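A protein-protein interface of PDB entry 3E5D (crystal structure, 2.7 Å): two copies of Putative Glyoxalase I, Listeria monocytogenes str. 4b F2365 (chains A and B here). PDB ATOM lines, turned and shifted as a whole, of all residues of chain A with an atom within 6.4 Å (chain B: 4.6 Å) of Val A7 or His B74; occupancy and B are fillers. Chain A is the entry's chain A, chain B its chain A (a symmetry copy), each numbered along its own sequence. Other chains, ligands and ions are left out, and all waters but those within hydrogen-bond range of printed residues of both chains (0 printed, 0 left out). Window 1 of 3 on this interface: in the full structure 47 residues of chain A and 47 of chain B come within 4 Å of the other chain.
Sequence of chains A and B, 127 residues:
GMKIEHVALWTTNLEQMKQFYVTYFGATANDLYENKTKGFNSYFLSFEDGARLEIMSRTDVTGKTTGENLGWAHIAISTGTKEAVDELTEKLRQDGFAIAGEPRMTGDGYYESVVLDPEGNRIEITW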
ATOM      1  N   ILE A   4       1.858  -5.303 -25.322  1.00  0.00           N
ATOM      2  CA  ILE A   4       0.852  -6.286 -25.714  1.00  0.00           C
ATOM      3  C   ILE A   4       0.407  -6.008 -27.140  1.00  0.00           C
ATOM      4  O   ILE A   4      -0.254  -5.012 -27.396  1.00  0.00           O
ATOM      5  CB  ILE A   4      -0.386  -6.237 -24.791  1.00  0.00           C
ATOM      6  CG1 ILE A   4      -0.010  -6.656 -23.365  1.00  0.00           C
ATOM      7  CG2 ILE A   4      -1.492  -7.137 -25.328  1.00  0.00           C
ATOM      8  CD1 ILE A   4      -1.192  -6.821 -22.433  1.00  0.00           C
ATOM      9  N   GLU A   5       0.757  -6.901 -28.063  1.00  0.00           N
ATOM     10  CA  GLU A   5       0.422  -6.725 -29.481  1.00  0.00           C
ATOM     11  C   GLU A   5      -1.027  -7.163 -29.731  1.00  0.00           C
ATOM     12  O   GLU A   5      -1.758  -6.502 -30.468  1.00  0.00           O
ATOM     13  CB  GLU A   5       1.437  -7.468 -30.380  1.00  0.00           C
ATOM     14  CG  GLU A   5       1.512  -6.987 -31.853  1.00  0.00           C
ATOM     15  CD  GLU A   5       0.316  -7.443 -32.710  1.00  0.00           C
ATOM     16  OE1 GLU A   5       0.180  -8.667 -32.989  1.00  0.00           O
ATOM     17  OE2 GLU A   5      -0.474  -6.562 -33.135  1.00  0.00           O
ATOM     18  N   HIS A   6      -1.448  -8.271 -29.132  1.00  0.00           N
ATOM     19  CA  HIS A   6      -2.832  -8.703 -29.291  1.00  0.00           C
ATOM     20  C   HIS A   6      -3.271  -9.666 -28.210  1.00  0.00           C
ATOM     21  O   HIS A   6      -2.459 -10.188 -27.458  1.00  0.00           O
ATOM     22  CB  HIS A   6      -3.079  -9.331 -30.674  1.00  0.00           C
ATOM     23  CG  HIS A   6      -2.435 -10.668 -30.873  1.00  0.00           C
ATOM     24  ND1 HIS A   6      -1.308 -10.843 -31.645  1.00  0.00           N
ATOM     25  CD2 HIS A   6      -2.778 -11.900 -30.427  1.00  0.00           C
ATOM     26  CE1 HIS A   6      -0.984 -12.125 -31.664  1.00  0.00           C
ATOM     27  NE2 HIS A   6      -1.857 -12.789 -30.927  1.00  0.00           N
ATOM     28  N   VAL A   7      -4.578  -9.861 -28.134  1.00  0.00           N
ATOM     29  CA  VAL A   7      -5.194 -10.829 -27.237  1.00  0.00           C
ATOM     30  C   VAL A   7      -6.022 -11.709 -28.180  1.00  0.00           C
ATOM     31  O   VAL A   7      -6.681 -11.185 -29.078  1.00  0.00           O
ATOM     32  CB  VAL A   7      -6.056 -10.160 -26.135  1.00  0.00           C
ATOM     33  CG1 VAL A   7      -6.952  -9.140 -26.725  1.00  0.00           C
ATOM     34  CG2 VAL A   7      -6.894 -11.183 -25.410  1.00  0.00           C
ATOM     35  N   ALA A   8      -5.959 -13.032 -27.996  1.00  0.00           N
ATOM     36  CA  ALA A   8      -6.622 -13.980 -28.890  1.00  0.00           C
ATOM     37  C   ALA A   8      -7.818 -14.659 -28.238  1.00  0.00           C
ATOM     38  O   ALA A   8      -7.823 -14.869 -27.033  1.00  0.00           O
ATOM     39  CB  ALA A   8      -5.629 -15.010 -29.359  1.00  0.00           C
ATOM     40  N   LEU A   9      -8.803 -15.039 -29.058  1.00  0.00           N
ATOM     41  CA  LEU A   9     -10.050 -15.652 -28.581  1.00  0.00           C
ATOM     42  C   LEU A   9     -10.476 -16.870 -29.407  1.00  0.00           C
ATOM     43  O   LEU A   9     -10.659 -16.755 -30.613  1.00  0.00           O
ATOM     44  CB  LEU A   9     -11.157 -14.595 -28.659  1.00  0.00           C
ATOM     45  CG  LEU A   9     -12.586 -14.898 -28.217  1.00  0.00           C
ATOM     46  CD1 LEU A   9     -12.628 -15.203 -26.727  1.00  0.00           C
ATOM     47  CD2 LEU A   9     -13.514 -13.727 -28.555  1.00  0.00           C
ATOM     48  N   TRP A  10     -10.622 -18.035 -28.766  1.00  0.00           N
ATOM     49  CA  TRP A  10     -11.110 -19.233 -29.462  1.00  0.00           C
ATOM     50  C   TRP A  10     -12.611 -19.102 -29.641  1.00  0.00           C
ATOM     51  O   TRP A  10     -13.365 -18.899 -28.689  1.00  0.00           O
ATOM     52  CB  TRP A  10     -10.779 -20.548 -28.747  1.00  0.00           C
ATOM     53  CG  TRP A  10      -9.398 -21.058 -29.006  1.00  0.00           C
ATOM     54  CD1 TRP A  10      -8.427 -21.278 -28.086  1.00  0.00           C
ATOM     55  CD2 TRP A  10      -8.832 -21.401 -30.277  1.00  0.00           C
ATOM     56  NE1 TRP A  10      -7.291 -21.753 -28.694  1.00  0.00           N
ATOM     57  CE2 TRP A  10      -7.511 -21.829 -30.043  1.00  0.00           C
ATOM     58  CE3 TRP A  10      -9.311 -21.386 -31.590  1.00  0.00           C
ATOM     59  CZ2 TRP A  10      -6.662 -22.238 -31.069  1.00  0.00           C
ATOM     60  CZ3 TRP A  10      -8.468 -21.798 -32.606  1.00  0.00           C
ATOM     61  CH2 TRP A  10      -7.158 -22.222 -32.338  1.00  0.00           C
ATOM     62  N   ALA A  51      -3.516  -2.728 -28.889  1.00  0.00           N
ATOM     63  CA  ALA A  51      -3.669  -4.155 -29.074  1.00  0.00           C
ATOM     64  C   ALA A  51      -4.829  -4.466 -29.990  1.00  0.00           C
ATOM     65  O   ALA A  51      -5.829  -3.740 -30.015  1.00  0.00           O
ATOM     66  CB  ALA A  51      -3.867  -4.851 -27.743  1.00  0.00           C
ATOM     67  N   ARG A  52      -4.651  -5.544 -30.748  1.00  0.00           N
ATOM     68  CA  ARG A  52      -5.659  -6.076 -31.635  1.00  0.00           C
ATOM     69  C   ARG A  52      -6.319  -7.275 -30.985  1.00  0.00           C
ATOM     70  O   ARG A  52      -5.806  -7.819 -30.002  1.00  0.00           O
ATOM     71  CB  ARG A  52      -5.019  -6.517 -32.938  1.00  0.00           C
ATOM     72  CG  ARG A  52      -4.460  -5.340 -33.714  1.00  0.00           C
ATOM     73  CD  ARG A  52      -4.044  -5.742 -35.090  1.00  0.00           C
ATOM     74  NE  ARG A  52      -2.907  -6.639 -35.008  1.00  0.00           N
ATOM     75  CZ  ARG A  52      -2.507  -7.438 -35.987  1.00  0.00           C
ATOM     76  NH1 ARG A  52      -3.163  -7.491 -37.143  1.00  0.00           N
ATOM     77  NH2 ARG A  52      -1.457  -8.218 -35.786  1.00  0.00           N
ATOM     78  N   LEU A  53      -7.464  -7.676 -31.527  1.00  0.00           N
ATOM     79  CA  LEU A  53      -8.163  -8.849 -31.048  1.00  0.00           C
ATOM     80  C   LEU A  53      -8.064  -9.888 -32.151  1.00  0.00           C
ATOM     81  O   LEU A  53      -8.453  -9.606 -33.285  1.00  0.00           O
ATOM     82  CB  LEU A  53      -9.617  -8.509 -30.762  1.00  0.00           C
ATOM     83  CG  LEU A  53     -10.554  -9.644 -30.335  1.00  0.00           C
ATOM     84  CD1 LEU A  53     -10.011 -10.422 -29.129  1.00  0.00           C
ATOM     85  CD2 LEU A  53     -11.946  -9.066 -30.046  1.00  0.00           C
ATOM     86  N   GLU A  54      -7.495 -11.055 -31.841  1.00  0.00           N
ATOM     87  CA  GLU A  54      -7.375 -12.144 -32.812  1.00  0.00           C
ATOM     88  C   GLU A  54      -8.486 -13.110 -32.526  1.00  0.00           C
ATOM     89  O   GLU A  54      -8.494 -13.748 -31.466  1.00  0.00           O
ATOM     90  CB  GLU A  54      -6.025 -12.879 -32.710  1.00  0.00           C
ATOM     91  CG  GLU A  54      -5.888 -14.041 -33.706  1.00  0.00           C
ATOM     92  CD  GLU A  54      -4.511 -14.720 -33.720  1.00  0.00           C
ATOM     93  OE1 GLU A  54      -3.680 -14.531 -32.787  1.00  0.00           O
ATOM     94  OE2 GLU A  54      -4.270 -15.465 -34.698  1.00  0.00           O
ATOM     95  N   ILE A  55      -9.452 -13.189 -33.436  1.00  0.00           N
ATOM     96  CA  ILE A  55     -10.550 -14.152 -33.275  1.00  0.00           C
ATOM     97  C   ILE A  55     -10.234 -15.325 -34.183  1.00  0.00           C
ATOM     98  O   ILE A  55      -9.938 -15.148 -35.370  1.00  0.00           O
ATOM     99  CB  ILE A  55     -11.962 -13.581 -33.537  1.00  0.00           C
ATOM    100  CG1 ILE A  55     -12.052 -12.886 -34.900  1.00  0.00           C
ATOM    101  CG2 ILE A  55     -12.334 -12.621 -32.436  1.00  0.00           C
ATOM    102  CD1 ILE A  55     -13.463 -12.436 -35.261  1.00  0.00           C
ATOM    103  N   MET A  56     -10.286 -16.524 -33.620  1.00  0.00           N
ATOM    104  CA  MET A  56      -9.919 -17.703 -34.365  1.00  0.00           C
ATOM    105  C   MET A  56     -10.788 -18.906 -34.032  1.00  0.00           C
ATOM    106  O   MET A  56     -11.496 -18.917 -33.036  1.00  0.00           O
ATOM    107  CB  MET A  56      -8.434 -17.982 -34.133  1.00  0.00           C
ATOM    108  CG  MET A  56      -8.020 -18.065 -32.673  1.00  0.00           C
ATOM    109  SD  MET A  56      -6.078 -17.852 -32.383  1.00  0.00           S
ATOM    110  CE  MET A  56      -6.090 -18.628 -30.501  1.00  0.00           C
ATOM    111  N   TRP A  72      -7.117 -16.737 -18.471  1.00  0.00           N
ATOM    112  CA  TRP A  72      -7.527 -15.447 -19.028  1.00  0.00           C
ATOM    113  C   TRP A  72      -8.969 -15.134 -18.645  1.00  0.00           C
ATOM    114  O   TRP A  72      -9.840 -15.946 -18.865  1.00  0.00           O
ATOM    115  CB  TRP A  72      -7.303 -15.434 -20.533  1.00  0.00           C
ATOM    116  CG  TRP A  72      -5.877 -15.685 -20.852  1.00  0.00           C
ATOM    117  CD1 TRP A  72      -5.356 -16.792 -21.428  1.00  0.00           C
ATOM    118  CD2 TRP A  72      -4.767 -14.831 -20.539  1.00  0.00           C
ATOM    119  NE1 TRP A  72      -3.988 -16.679 -21.530  1.00  0.00           N
ATOM    120  CE2 TRP A  72      -3.600 -15.485 -20.988  1.00  0.00           C
ATOM    121  CE3 TRP A  72      -4.648 -13.568 -19.941  1.00  0.00           C
ATOM    122  CZ2 TRP A  72      -2.325 -14.925 -20.856  1.00  0.00           C
ATOM    123  CZ3 TRP A  72      -3.378 -13.008 -19.808  1.00  0.00           C
ATOM    124  CH2 TRP A  72      -2.234 -13.687 -20.266  1.00  0.00           C
ATOM    125  N   HIS A  74     -10.957 -11.655 -18.947  1.00  0.00           N
ATOM    126  CA  HIS A  74     -11.770 -10.796 -19.802  1.00  0.00           C
ATOM    127  C   HIS A  74     -10.896  -9.791 -20.523  1.00  0.00           C
ATOM    128  O   HIS A  74      -9.678  -9.800 -20.386  1.00  0.00           O
ATOM    129  CB  HIS A  74     -12.818 -10.040 -18.956  1.00  0.00           C
ATOM    130  CG  HIS A  74     -12.236  -9.086 -17.943  1.00  0.00           C
ATOM    131  ND1 HIS A  74     -12.144  -9.387 -16.600  1.00  0.00           N
ATOM    132  CD2 HIS A  74     -11.739  -7.828 -18.081  1.00  0.00           C
ATOM    133  CE1 HIS A  74     -11.604  -8.362 -15.959  1.00  0.00           C
ATOM    134  NE2 HIS A  74     -11.346  -7.403 -16.834  1.00  0.00           N
ATOM    135  N   ILE A  75     -11.512  -8.944 -21.327  1.00  0.00           N
ATOM    136  CA  ILE A  75     -10.788  -7.830 -21.912  1.00  0.00           C
ATOM    137  C   ILE A  75     -11.656  -6.608 -21.620  1.00  0.00           C
ATOM    138  O   ILE A  75     -12.855  -6.735 -21.384  1.00  0.00           O
ATOM    139  CB  ILE A  75     -10.447  -8.006 -23.421  1.00  0.00           C
ATOM    140  CG1 ILE A  75     -11.681  -7.894 -24.312  1.00  0.00           C
ATOM    141  CG2 ILE A  75      -9.754  -9.334 -23.669  1.00  0.00           C
ATOM    142  CD1 ILE A  75     -11.321  -7.866 -25.796  1.00  0.00           C
ATOM    143  N   ILE B   4      -8.695  -1.376 -26.780  1.00  0.00           N
ATOM    144  CA  ILE B   4      -8.507  -2.337 -25.697  1.00  0.00           C
ATOM    145  C   ILE B   4      -7.677  -1.699 -24.596  1.00  0.00           C
ATOM    146  O   ILE B   4      -6.493  -1.455 -24.782  1.00  0.00           O
ATOM    147  CB  ILE B   4      -7.787  -3.614 -26.183  1.00  0.00           C
ATOM    148  CG1 ILE B   4      -8.659  -4.372 -27.191  1.00  0.00           C
ATOM    149  CG2 ILE B   4      -7.440  -4.516 -25.005  1.00  0.00           C
ATOM    150  CD1 ILE B   4      -8.119  -5.733 -27.581  1.00  0.00           C
ATOM    151  N   VAL B   7      -6.310  -6.435 -20.549  1.00  0.00           N
ATOM    152  CA  VAL B   7      -6.694  -7.839 -20.604  1.00  0.00           C
ATOM    153  C   VAL B   7      -6.443  -8.330 -19.173  1.00  0.00           C
ATOM    154  O   VAL B   7      -5.418  -7.986 -18.584  1.00  0.00           O
ATOM    155  CB  VAL B   7      -5.886  -8.640 -21.658  1.00  0.00           C
ATOM    156  CG1 VAL B   7      -4.440  -8.353 -21.533  1.00  0.00           C
ATOM    157  CG2 VAL B   7      -6.105 -10.123 -21.493  1.00  0.00           C
ATOM    158  N   TRP B  72     -11.125 -17.017 -24.008  1.00  0.00           N
ATOM    159  CA  TRP B  72      -9.866 -16.289 -24.168  1.00  0.00           C
ATOM    160  C   TRP B  72      -8.701 -17.262 -24.316  1.00  0.00           C
ATOM    161  O   TRP B  72      -8.542 -18.139 -23.495  1.00  0.00           O
ATOM    162  CB  TRP B  72      -9.674 -15.317 -23.013  1.00  0.00           C
ATOM    163  CG  TRP B  72     -10.801 -14.355 -22.947  1.00  0.00           C
ATOM    164  CD1 TRP B  72     -11.763 -14.296 -21.998  1.00  0.00           C
ATOM    165  CD2 TRP B  72     -11.129 -13.352 -23.919  1.00  0.00           C
ATOM    166  NE1 TRP B  72     -12.662 -13.296 -22.292  1.00  0.00           N
ATOM    167  CE2 TRP B  72     -12.298 -12.703 -23.469  1.00  0.00           C
ATOM    168  CE3 TRP B  72     -10.536 -12.927 -25.117  1.00  0.00           C
ATOM    169  CZ2 TRP B  72     -12.893 -11.652 -24.173  1.00  0.00           C
ATOM    170  CZ3 TRP B  72     -11.129 -11.880 -25.822  1.00  0.00           C
ATOM    171  CH2 TRP B  72     -12.295 -11.254 -25.345  1.00  0.00           C
ATOM    172  N   ALA B  73      -7.903 -17.098 -25.372  1.00  0.00           N
ATOM    173  CA  ALA B  73      -6.833 -18.051 -25.726  1.00  0.00           C
ATOM    174  C   ALA B  73      -5.424 -17.726 -25.222  1.00  0.00           C
ATOM    175  O   ALA B  73      -4.771 -18.582 -24.624  1.00  0.00           O
ATOM    176  CB  ALA B  73      -6.794 -18.225 -27.239  1.00  0.00           C
ATOM    177  N   HIS B  74      -4.937 -16.525 -25.513  1.00  0.00           N
ATOM    178  CA  HIS B  74      -3.594 -16.125 -25.104  1.00  0.00           C
ATOM    179  C   HIS B  74      -3.415 -14.631 -25.273  1.00  0.00           C
ATOM    180  O   HIS B  74      -4.338 -13.923 -25.658  1.00  0.00           O
ATOM    181  CB  HIS B  74      -2.538 -16.860 -25.958  1.00  0.00           C
ATOM    182  CG  HIS B  74      -2.576 -16.527 -27.429  1.00  0.00           C
ATOM    183  ND1 HIS B  74      -3.147 -17.361 -28.369  1.00  0.00           N
ATOM    184  CD2 HIS B  74      -2.094 -15.459 -28.118  1.00  0.00           C
ATOM    185  CE1 HIS B  74      -3.024 -16.814 -29.569  1.00  0.00           C
ATOM    186  NE2 HIS B  74      -2.391 -15.658 -29.445  1.00  0.00           N
ATOM    187  N   ILE B  75      -2.234 -14.138 -24.945  1.00  0.00           N
ATOM    188  CA  ILE B  75      -1.907 -12.757 -25.246  1.00  0.00           C
ATOM    189  C   ILE B  75      -0.553 -12.824 -25.949  1.00  0.00           C
ATOM    190  O   ILE B  75       0.184 -13.796 -25.795  1.00  0.00           O
ATOM    191  CB  ILE B  75      -1.922 -11.808 -24.012  1.00  0.00           C
ATOM    192  CG1 ILE B  75      -0.748 -12.060 -23.072  1.00  0.00           C
ATOM    193  CG2 ILE B  75      -3.228 -11.934 -23.248  1.00  0.00           C
ATOM    194  CD1 ILE B  75      -0.651 -11.002 -21.974  1.00  0.00           C
ATOM    195  N   ALA B  76      -0.247 -11.832 -26.768  1.00  0.00           N
ATOM    196  CA  ALA B  76       1.014 -11.806 -27.467  1.00  0.00           C
ATOM    197  C   ALA B  76       1.743 -10.540 -27.034  1.00  0.00           C
ATOM    198  O   ALA B  76       1.164  -9.456 -27.106  1.00  0.00           O
ATOM    199  CB  ALA B  76       0.779 -11.817 -28.971  1.00  0.00           C
ATOM    200  N   ARG B 122      -0.774 -19.358 -21.796  1.00  0.00           N
ATOM    201  CA  ARG B 122      -0.011 -19.164 -23.042  1.00  0.00           C
ATOM    202  C   ARG B 122       0.305 -17.714 -23.330  1.00  0.00           C
ATOM    203  O   ARG B 122      -0.555 -16.859 -23.217  1.00  0.00           O
ATOM    204  CB  ARG B 122      -0.772 -19.721 -24.246  1.00  0.00           C
ATOM    205  CG  ARG B 122      -0.994 -21.224 -24.185  1.00  0.00           C
ATOM    206  CD  ARG B 122      -1.881 -21.715 -25.321  1.00  0.00           C
ATOM    207  NE  ARG B 122      -1.364 -21.285 -26.625  1.00  0.00           N
ATOM    208  CZ  ARG B 122      -0.494 -21.972 -27.363  1.00  0.00           C
ATOM    209  NH1 ARG B 122      -0.016 -23.147 -26.948  1.00  0.00           N
ATOM    210  NH2 ARG B 122      -0.098 -21.476 -28.530  1.00  0.00           N
ATOM    211  N   GLU B 124       2.424 -15.622 -26.447  1.00  0.00           N
ATOM    212  CA  GLU B 124       3.183 -15.652 -27.692  1.00  0.00           C
ATOM    213  C   GLU B 124       4.181 -14.530 -27.564  1.00  0.00           C
ATOM    214  O   GLU B 124       3.790 -13.413 -27.273  1.00  0.00           O
ATOM    215  CB  GLU B 124       2.300 -15.406 -28.921  1.00  0.00           C
ATOM    216  CG  GLU B 124       1.384 -16.557 -29.286  1.00  0.00           C
ATOM    217  CD  GLU B 124       0.518 -16.301 -30.531  1.00  0.00           C
ATOM    218  OE1 GLU B 124       0.475 -15.165 -31.041  1.00  0.00           O
ATOM    219  OE2 GLU B 124      -0.143 -17.254 -31.000  1.00  0.00           O
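A ring nitrogen (NE2) of His A6 sits at hydrogen-bond distance from a ring nitrogen (NE2) of His B74, 3.3 Å away.
The backbone NH (N) of Ala B73 is in hydrogen-bond range of the backbone carbonyl oxygen (O) of Ala A8.
N of Ala A8 sits at hydrogen-bond distance from O of His B74, at 3.0 Å.
NE2 of His A6 is in hydrogen-bond range of OE1 of Glu B124, at 3.3 Å.
O of Ala B76 is in hydrogen-bond range of N of Glu A5 (2.8 Å).
The backbone carbonyl oxygen (O) of His A6 sits at hydrogen-bond distance from the backbone NH (N) of Ala B76 (2.8 Å).
Ile A4 touches Val B7, and with the chains exchanged Val A7 touches Ile B4.
Val A7 touches His B74, and with the chains exchanged His A74 touches Val B7.
Trp B72 touches its own counterpart, Trp A72.
Trp A72 touches Ile B75, and with the chains exchanged Ile A75 touches Trp B72.
Of the 28 pairs that touch across the chains among the printed residues, 9 have their exchanged pair printed and touching as well.
Of the 9 printed residues of chain B, 9 touch a printed residue of chain A.
Of the 16 printed residues of chain A, 15 touch a printed residue of chain B.
Printed residues of chain A that touch a printed residue of chain B: Ile A4, Glu A5, His A6, Val A7, Ala A8, Leu A9, Trp A10, Ala A51, Arg A52, Leu A53, Glu A54, Met A56, Trp A72, His A74 and Ile A75.
Hydrophobic or aromatic side chains of chain A that line the printed part of chain B: Ile A4, His A6, Val A7, Ala A8, Leu A9, Trp A10, Leu A53, Met A56, Trp A72 and Ile A75.
Among the printed residues, 28 pairs touch across the chains.
OE1 of Glu A54 sits at hydrogen-bond distance from NE2 of His A6.
O of Val A7 lies within hydrogen-bond range of N of Glu A54.
The side-chain carboxylate (OE1) of Glu A5 lies within hydrogen-bond range of a ring nitrogen (ND1) of His A6 (3.0 Å).
N of Val A7 is in hydrogen-bond range of O of Arg A52 (3.0 Å).
The backbone carbonyl oxygen of Ile B75 sits at hydrogen-bond distance from the backbone NH of Glu B124 (3.0 Å).
The side-chain carboxylate (OE2) of Glu A5 is in salt-bridge range of the guanidinium group (NE) of Arg A52 (3.1 Å).
Among the printed residues, pairs that only touch across the chains: Met A56 with Ala B73, Trp A72 with Trp B72, His A6 with Ile B75, Ile A4 with Ala B76, Leu A9 with Trp B72, Trp A72 with Arg B122, Ile A75 with Trp B72, Trp A72 with Ile B75, Trp A10 with Ala B73, His A74 with Val B7, Val A7 with His B74, Trp A72 with His B74, His A74 with Trp B72, Met A56 with His B74, Val A7 with Ile B4, Ile A4 with Val B7, Trp A72 with Ala B73, Ala A8 with Trp B72, Glu A54 with His B74, Leu A53 with Trp B72, Ala A51 with Ile B4 and Arg A52 with Ile B4.
Of chain B, only Ile B4 (3.7 Å) and His B74 (3.6 Å) come within 4 Å of Val A7.
Of chain A, only His A6 (3.3 Å), Val A7 (3.6 Å), Ala A8 (3.0 Å), Glu A54 (3.8 Å), Met A56 (3.7 Å) and Trp A72 (3.6 Å) come within 4 Å of His B74.
Printed residues of chain B within 4 Å of Glu A54: His B74.
Of the printed residues of chain B, Ile A75 touches Trp B72 (3.6 Å).
Printed residues of chain B within 4 Å of Leu A53: Trp B72.
Of the printed residues of chain A, Ala B73 touches Ala A8, Trp A10, Met A56 and Trp A72.
Ile A55 touches none of the printed residues of chain B.
The nearest residue of chain B that does not touch Val A7 is Trp B72 (4.05 Å).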
